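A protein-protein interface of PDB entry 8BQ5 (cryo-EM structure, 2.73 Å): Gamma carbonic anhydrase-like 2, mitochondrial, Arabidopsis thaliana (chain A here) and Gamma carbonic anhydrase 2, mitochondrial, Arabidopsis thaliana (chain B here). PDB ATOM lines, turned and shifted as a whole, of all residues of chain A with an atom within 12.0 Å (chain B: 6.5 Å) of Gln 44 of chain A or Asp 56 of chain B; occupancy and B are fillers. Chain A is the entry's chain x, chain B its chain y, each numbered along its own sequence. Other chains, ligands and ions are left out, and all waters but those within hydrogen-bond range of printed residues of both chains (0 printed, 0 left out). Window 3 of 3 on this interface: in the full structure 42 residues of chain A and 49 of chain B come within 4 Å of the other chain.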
ATOM      1  N   GLN A  44      17.770  20.771 -23.783  1.00  0.00           N
ATOM      2  CA  GLN A  44      16.788  21.847 -23.834  1.00  0.00           C
ATOM      3  C   GLN A  44      17.091  22.923 -22.796  1.00  0.00           C
ATOM      4  O   GLN A  44      17.369  22.615 -21.637  1.00  0.00           O
ATOM      5  CB  GLN A  44      15.378  21.298 -23.616  1.00  0.00           C
ATOM      6  CG  GLN A  44      14.284  22.266 -24.026  1.00  0.00           C
ATOM      7  CD  GLN A  44      12.998  22.058 -23.255  1.00  0.00           C
ATOM      8  OE1 GLN A  44      13.019  21.703 -22.077  1.00  0.00           O
ATOM      9  NE2 GLN A  44      11.870  22.298 -23.910  1.00  0.00           N
ATOM     10  N   VAL A  45      17.037  24.182 -23.217  1.00  0.00           N
ATOM     11  CA  VAL A  45      17.257  25.325 -22.338  1.00  0.00           C
ATOM     12  C   VAL A  45      15.886  25.771 -21.840  1.00  0.00           C
ATOM     13  O   VAL A  45      15.135  26.436 -22.558  1.00  0.00           O
ATOM     14  CB  VAL A  45      18.001  26.457 -23.050  1.00  0.00           C
ATOM     15  CG1 VAL A  45      18.094  27.682 -22.155  1.00  0.00           C
ATOM     16  CG2 VAL A  45      19.389  25.999 -23.464  1.00  0.00           C
ATOM     17  N   THR A  46      15.558  25.409 -20.599  1.00  0.00           N
ATOM     18  CA  THR A  46      14.251  25.710 -20.038  1.00  0.00           C
ATOM     19  C   THR A  46      14.381  26.831 -19.020  1.00  0.00           C
ATOM     20  O   THR A  46      14.930  26.604 -17.931  1.00  0.00           O
ATOM     21  CB  THR A  46      13.648  24.467 -19.387  1.00  0.00           C
ATOM     22  OG1 THR A  46      13.675  23.381 -20.320  1.00  0.00           O
ATOM     23  CG2 THR A  46      12.210  24.731 -18.976  1.00  0.00           C
ATOM     24  N   PRO A  47      13.898  28.035 -19.310  1.00  0.00           N
ATOM     25  CA  PRO A  47      14.066  29.153 -18.380  1.00  0.00           C
ATOM     26  C   PRO A  47      13.087  29.077 -17.215  1.00  0.00           C
ATOM     27  O   PRO A  47      12.112  28.325 -17.224  1.00  0.00           O
ATOM     28  CB  PRO A  47      13.786  30.378 -19.254  1.00  0.00           C
ATOM     29  CG  PRO A  47      12.837  29.878 -20.283  1.00  0.00           C
ATOM     30  CD  PRO A  47      13.200  28.438 -20.543  1.00  0.00           C
ATOM     31  N   SER A  48      13.368  29.891 -16.199  1.00  0.00           N
ATOM     32  CA  SER A  48      12.486  30.026 -15.054  1.00  0.00           C
ATOM     33  C   SER A  48      11.913  31.431 -15.013  1.00  0.00           C
ATOM     34  O   SER A  48      12.665  32.405 -15.163  1.00  0.00           O
ATOM     35  CB  SER A  48      13.230  29.729 -13.748  1.00  0.00           C
ATOM     36  OG  SER A  48      13.870  30.888 -13.245  1.00  0.00           O
ATOM     37  N   PRO A  49      10.599  31.581 -14.836  1.00  0.00           N
ATOM     38  CA  PRO A  49      10.013  32.931 -14.803  1.00  0.00           C
ATOM     39  C   PRO A  49      10.479  33.770 -13.629  1.00  0.00           C
ATOM     40  O   PRO A  49      10.534  34.999 -13.754  1.00  0.00           O
ATOM     41  CB  PRO A  49       8.501  32.662 -14.725  1.00  0.00           C
ATOM     42  CG  PRO A  49       8.334  31.205 -15.073  1.00  0.00           C
ATOM     43  CD  PRO A  49       9.587  30.537 -14.619  1.00  0.00           C
ATOM     44  N   ASP A  50      10.819  33.156 -12.501  1.00  0.00           N
ATOM     45  CA  ASP A  50      11.130  33.901 -11.291  1.00  0.00           C
ATOM     46  C   ASP A  50      12.602  34.274 -11.171  1.00  0.00           C
ATOM     47  O   ASP A  50      13.002  34.809 -10.132  1.00  0.00           O
ATOM     48  CB  ASP A  50      10.692  33.109 -10.053  1.00  0.00           C
ATOM     49  CG  ASP A  50      11.363  31.755  -9.957  1.00  0.00           C
ATOM     50  OD1 ASP A  50      11.985  31.323 -10.949  1.00  0.00           O
ATOM     51  OD2 ASP A  50      11.271  31.125  -8.882  1.00  0.00           O
ATOM     52  N   ARG A  51      13.418  34.006 -12.188  1.00  0.00           N
ATOM     53  CA  ARG A  51      14.811  34.432 -12.141  1.00  0.00           C
ATOM     54  C   ARG A  51      14.896  35.952 -12.204  1.00  0.00           C
ATOM     55  O   ARG A  51      14.243  36.595 -13.030  1.00  0.00           O
ATOM     56  CB  ARG A  51      15.616  33.808 -13.284  1.00  0.00           C
ATOM     57  CG  ARG A  51      16.897  34.572 -13.620  1.00  0.00           C
ATOM     58  CD  ARG A  51      17.633  33.995 -14.818  1.00  0.00           C
ATOM     59  NE  ARG A  51      18.002  32.595 -14.639  1.00  0.00           N
ATOM     60  CZ  ARG A  51      19.071  32.178 -13.973  1.00  0.00           C
ATOM     61  NH1 ARG A  51      19.899  33.029 -13.390  1.00  0.00           N
ATOM     62  NH2 ARG A  51      19.315  30.874 -13.889  1.00  0.00           N
ATOM     63  N   VAL A  52      15.713  36.523 -11.322  1.00  0.00           N
ATOM     64  CA  VAL A  52      15.796  37.972 -11.181  1.00  0.00           C
ATOM     65  C   VAL A  52      16.568  38.550 -12.359  1.00  0.00           C
ATOM     66  O   VAL A  52      17.693  38.129 -12.652  1.00  0.00           O
ATOM     67  CB  VAL A  52      16.453  38.351  -9.847  1.00  0.00           C
ATOM     68  CG1 VAL A  52      16.714  39.849  -9.779  1.00  0.00           C
ATOM     69  CG2 VAL A  52      15.583  37.902  -8.689  1.00  0.00           C
ATOM     70  N   LYS A  53      15.987  39.504 -13.077  1.00  0.00           N
ATOM     71  CA  LYS A  53      16.692  40.186 -14.196  1.00  0.00           C
ATOM     72  C   LYS A  53      17.323  41.481 -13.671  1.00  0.00           C
ATOM     73  O   LYS A  53      18.392  41.842 -14.172  1.00  0.00           O
ATOM     74  CB  LYS A  53      15.710  40.456 -15.338  1.00  0.00           C
ATOM     75  CG  LYS A  53      15.314  39.238 -16.160  1.00  0.00           C
ATOM     76  CD  LYS A  53      14.497  39.576 -17.389  1.00  0.00           C
ATOM     77  CE  LYS A  53      15.097  40.680 -18.235  1.00  0.00           C
ATOM     78  NZ  LYS A  53      15.405  40.225 -19.611  1.00  0.00           N
ATOM     79  N   LEU B  54      18.240  33.709 -23.075  1.00  0.00           N
ATOM     80  CA  LEU B  54      17.545  32.473 -22.734  1.00  0.00           C
ATOM     81  C   LEU B  54      18.422  31.689 -21.765  1.00  0.00           C
ATOM     82  O   LEU B  54      19.364  31.010 -22.183  1.00  0.00           O
ATOM     83  CB  LEU B  54      17.240  31.662 -23.991  1.00  0.00           C
ATOM     84  CG  LEU B  54      16.320  30.452 -23.828  1.00  0.00           C
ATOM     85  CD1 LEU B  54      15.017  30.860 -23.160  1.00  0.00           C
ATOM     86  CD2 LEU B  54      16.057  29.793 -25.174  1.00  0.00           C
ATOM     87  N   VAL B  55      18.106  31.779 -20.475  1.00  0.00           N
ATOM     88  CA  VAL B  55      18.915  31.188 -19.415  1.00  0.00           C
ATOM     89  C   VAL B  55      18.129  30.055 -18.776  1.00  0.00           C
ATOM     90  O   VAL B  55      16.976  30.241 -18.372  1.00  0.00           O
ATOM     91  CB  VAL B  55      19.320  32.232 -18.359  1.00  0.00           C
ATOM     92  CG1 VAL B  55      20.412  31.680 -17.461  1.00  0.00           C
ATOM     93  CG2 VAL B  55      19.781  33.508 -19.031  1.00  0.00           C
ATOM     94  N   ASP B  56      18.763  28.891 -18.669  1.00  0.00           N
ATOM     95  CA  ASP B  56      18.123  27.723 -18.087  1.00  0.00           C
ATOM     96  C   ASP B  56      17.868  27.949 -16.596  1.00  0.00           C
ATOM     97  O   ASP B  56      18.414  28.864 -15.975  1.00  0.00           O
ATOM     98  CB  ASP B  56      18.997  26.488 -18.312  1.00  0.00           C
ATOM     99  CG  ASP B  56      18.271  25.192 -18.025  1.00  0.00           C
ATOM    100  OD1 ASP B  56      17.864  24.519 -18.996  1.00  0.00           O
ATOM    101  OD2 ASP B  56      18.118  24.835 -16.838  1.00  0.00           O
ATOM    102  N   LYS B  57      17.010  27.100 -16.026  1.00  0.00           N
ATOM    103  CA  LYS B  57      16.585  27.248 -14.638  1.00  0.00           C
ATOM    104  C   LYS B  57      17.750  27.210 -13.654  1.00  0.00           C
ATOM    105  O   LYS B  57      17.920  28.119 -12.835  1.00  0.00           O
ATOM    106  CB  LYS B  57      15.580  26.142 -14.300  1.00  0.00           C
ATOM    107  CG  LYS B  57      14.888  26.307 -12.961  1.00  0.00           C
ATOM    108  CD  LYS B  57      13.378  26.241 -13.100  1.00  0.00           C
ATOM    109  CE  LYS B  57      12.710  26.203 -11.736  1.00  0.00           C
ATOM    110  NZ  LYS B  57      13.357  25.205 -10.834  1.00  0.00           N
ATOM    111  N   ASP B  58      18.560  26.161 -13.715  1.00  0.00           N
ATOM    112  CA  ASP B  58      19.655  25.981 -12.761  1.00  0.00           C
ATOM    113  C   ASP B  58      20.981  26.439 -13.366  1.00  0.00           C
ATOM    114  O   ASP B  58      21.917  25.668 -13.579  1.00  0.00           O
ATOM    115  CB  ASP B  58      19.716  24.532 -12.292  1.00  0.00           C
ATOM    116  CG  ASP B  58      19.885  23.563 -13.429  1.00  0.00           C
ATOM    117  OD1 ASP B  58      18.995  23.527 -14.300  1.00  0.00           O
ATOM    118  OD2 ASP B  58      20.904  22.841 -13.452  1.00  0.00           O
ATOM    119  N   VAL B  59      21.042  27.736 -13.642  1.00  0.00           N
ATOM    120  CA  VAL B  59      22.257  28.400 -14.089  1.00  0.00           C
ATOM    121  C   VAL B  59      22.588  29.482 -13.077  1.00  0.00           C
ATOM    122  O   VAL B  59      21.740  30.327 -12.768  1.00  0.00           O
ATOM    123  CB  VAL B  59      22.096  29.003 -15.496  1.00  0.00           C
ATOM    124  CG1 VAL B  59      23.308  29.851 -15.858  1.00  0.00           C
ATOM    125  CG2 VAL B  59      21.892  27.908 -16.514  1.00  0.00           C
ATOM    126  N   PHE B  60      23.808  29.454 -12.553  1.00  0.00           N
ATOM    127  CA  PHE B  60      24.257  30.530 -11.683  1.00  0.00           C
ATOM    128  C   PHE B  60      24.713  31.702 -12.536  1.00  0.00           C
ATOM    129  O   PHE B  60      25.702  31.600 -13.267  1.00  0.00           O
ATOM    130  CB  PHE B  60      25.391  30.080 -10.767  1.00  0.00           C
ATOM    131  CG  PHE B  60      26.019  31.209  -9.999  1.00  0.00           C
ATOM    132  CD1 PHE B  60      25.231  32.111  -9.301  1.00  0.00           C
ATOM    133  CD2 PHE B  60      27.388  31.389  -9.999  1.00  0.00           C
ATOM    134  CE1 PHE B  60      25.801  33.154  -8.602  1.00  0.00           C
ATOM    135  CE2 PHE B  60      27.963  32.435  -9.302  1.00  0.00           C
ATOM    136  CZ  PHE B  60      27.167  33.317  -8.603  1.00  0.00           C
ATOM    137  N   ILE B  73      22.148  30.057 -22.585  1.00  0.00           N
ATOM    138  CA  ILE B  73      22.986  29.383 -21.601  1.00  0.00           C
ATOM    139  C   ILE B  73      22.267  28.123 -21.138  1.00  0.00           C
ATOM    140  O   ILE B  73      21.093  28.178 -20.757  1.00  0.00           O
ATOM    141  CB  ILE B  73      23.320  30.300 -20.409  1.00  0.00           C
ATOM    142  CG1 ILE B  73      23.978  31.590 -20.899  1.00  0.00           C
ATOM    143  CG2 ILE B  73      24.249  29.600 -19.442  1.00  0.00           C
ATOM    144  CD1 ILE B  73      23.903  32.728 -19.912  1.00  0.00           C
ATOM    145  N   GLY B  74      22.976  26.991 -21.167  1.00  0.00           N
ATOM    146  CA  GLY B  74      22.372  25.702 -20.918  1.00  0.00           C
ATOM    147  C   GLY B  74      22.475  25.242 -19.473  1.00  0.00           C
ATOM    148  O   GLY B  74      23.099  25.874 -18.623  1.00  0.00           O
ATOM    149  N   LYS B  75      21.860  24.088 -19.221  1.00  0.00           N
ATOM    150  CA  LYS B  75      21.694  23.564 -17.870  1.00  0.00           C
ATOM    151  C   LYS B  75      23.033  23.322 -17.184  1.00  0.00           C
ATOM    152  O   LYS B  75      23.968  22.782 -17.779  1.00  0.00           O
ATOM    153  CB  LYS B  75      20.898  22.258 -17.929  1.00  0.00           C
ATOM    154  CG  LYS B  75      20.588  21.637 -16.586  1.00  0.00           C
ATOM    155  CD  LYS B  75      19.755  20.376 -16.746  1.00  0.00           C
ATOM    156  CE  LYS B  75      19.460  19.731 -15.400  1.00  0.00           C
ATOM    157  NZ  LYS B  75      18.645  18.493 -15.532  1.00  0.00           N
ATOM    158  N   GLY B  76      23.115  23.716 -15.915  1.00  0.00           N
ATOM    159  CA  GLY B  76      24.294  23.485 -15.109  1.00  0.00           C
ATOM    160  C   GLY B  76      25.425  24.464 -15.321  1.00  0.00           C
ATOM    161  O   GLY B  76      26.467  24.333 -14.666  1.00  0.00           O
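The backbone NH (N) of Asp 56 of chain B is in hydrogen-bond range of the backbone carbonyl oxygen (O) of Ile 73 of chain B (3.2 Å). The side-chain amide oxygen (OE1) of Gln 44 of chain A lies within hydrogen-bond range of the side-chain hydroxyl (OG1) of Thr 46 of chain A, 2.5 Å away. The backbone NH (N) of Asp 58 of chain B sits at hydrogen-bond distance from the side-chain carboxylate (OD2) of Asp 56 of chain B (3.4 Å). The side-chain hydroxyl (OG) of Ser 48 of chain A is in hydrogen-bond range of the backbone NH (N) of Arg 51 of chain A. The backbone NH (N) of Ile 73 of chain B sits at hydrogen-bond distance from the backbone carbonyl oxygen (O) of Leu 54 of chain B, 3.0 Å away. The side-chain hydroxyl of Ser 48 of chain A sits at hydrogen-bond distance from the side-chain carboxylate of Asp 50 of chain A (3.0 Å).
Gln 44 of chain A touches just one residue of chain B: Asp 56. Printed residues of chain B within 4 Å of Thr 46 of chain A: Asp 56 (2.9 Å) and Lys 57 (2.9 Å). Of the printed residues of chain B, Pro 47 of chain A touches Leu 54 and Val 55. Printed residues of chain B within 4 Å of Arg 51 of chain A: Val 55, Asp 56, Lys 57 and Val 59. Val 52 of chain A touches none of the printed residues of chain B. Of chain A, only Val 45 and Pro 47 come within 4 Å of Leu 54 of chain B. Of chain A, only Pro 47 (3.1 Å) and Arg 51 (3.8 Å) come within 4 Å of Val 55 of chain B. Printed residues of chain A within 4 Å of Asp 56 of chain B: Gln 44, Val 45, Thr 46 and Arg 51. Lys 57 of chain B touches three residues of chain A. Asp 58 of chain B touches none of the printed residues of chain A. Of chain A, only Arg 51 (2.7 Å) comes within 4 Å of Val 59 of chain B. Phe 60 of chain B touches none of the printed residues of chain A. Of chain A, only Val 45 comes within 4 Å of Ile 73 of chain B. Of chain A, only Val 45 (3.9 Å) comes within 4 Å of Gly 74 of chain B. Lys 75 of chain B touches none of the printed residues of chain A. The nearest residue of chain B that does not touch Gln 44 of chain A is Lys 75 of chain B (5.1 Å). The nearest residue of chain A that does not touch Asp 56 of chain B is Pro 47 of chain A (4.3 Å).
CG1 of Val 45 of chain A touches O of Leu 54 of chain B, at 3.6 Å. Val 45 of chain A touches Asp 56 of chain B (CA to OD1, 3.5 Å). Val 45 of chain A touches Ile 73 of chain B (CG1 to O, 3.3 Å). Gly 74 of chain B touches Val 45 of chain A. CD1 of Leu 54 of chain B touches CG of Pro 47 of chain A, 3.7 Å away. Val 55 of chain B touches Pro 47 of chain A. CB of Ser 48 of chain A touches CD of Lys 57 of chain B, 3.6 Å away. CZ of Arg 51 of chain A touches CG1 of Val 55 of chain B, at 3.8 Å.
Hydrophobic or aromatic side chains of chain A that line the printed part of chain B: Val 45 and Pro 47. Of the 11 printed residues of chain B, 7 touch a printed residue of chain A. Printed residues of chain B that touch a printed residue of chain A: Leu 54, Val 55, Asp 56, Lys 57, Val 59, Ile 73 and Gly 74. Among the printed residues, 14 pairs touch across the chains.
The guanidinium group of Arg 51 of chain A is in hydrogen-bond range of the backbone carbonyl oxygen of Lys 57 of chain B, 3.3 Å away. O of Thr 46 of chain A lies within hydrogen-bond range of N of Lys 57 of chain B. The backbone carbonyl oxygen (O) of Val 59 of chain B is in hydrogen-bond range of the guanidinium group (NH2) of Arg 51 of chain A, at 2.7 Å. The backbone carbonyl oxygen (O) of Asp 56 of chain B is in hydrogen-bond range of the guanidinium group (NH2) of Arg 51 of chain A (3.0 Å). O of Gln 44 of chain A lies close to OD1 of Asp 56 of chain B, at 3.3 Å. The side-chain carboxylate (OD1) of Asp 56 of chain B is in hydrogen-bond range of the backbone NH (N) of Thr 46 of chain A, 2.9 Å away.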
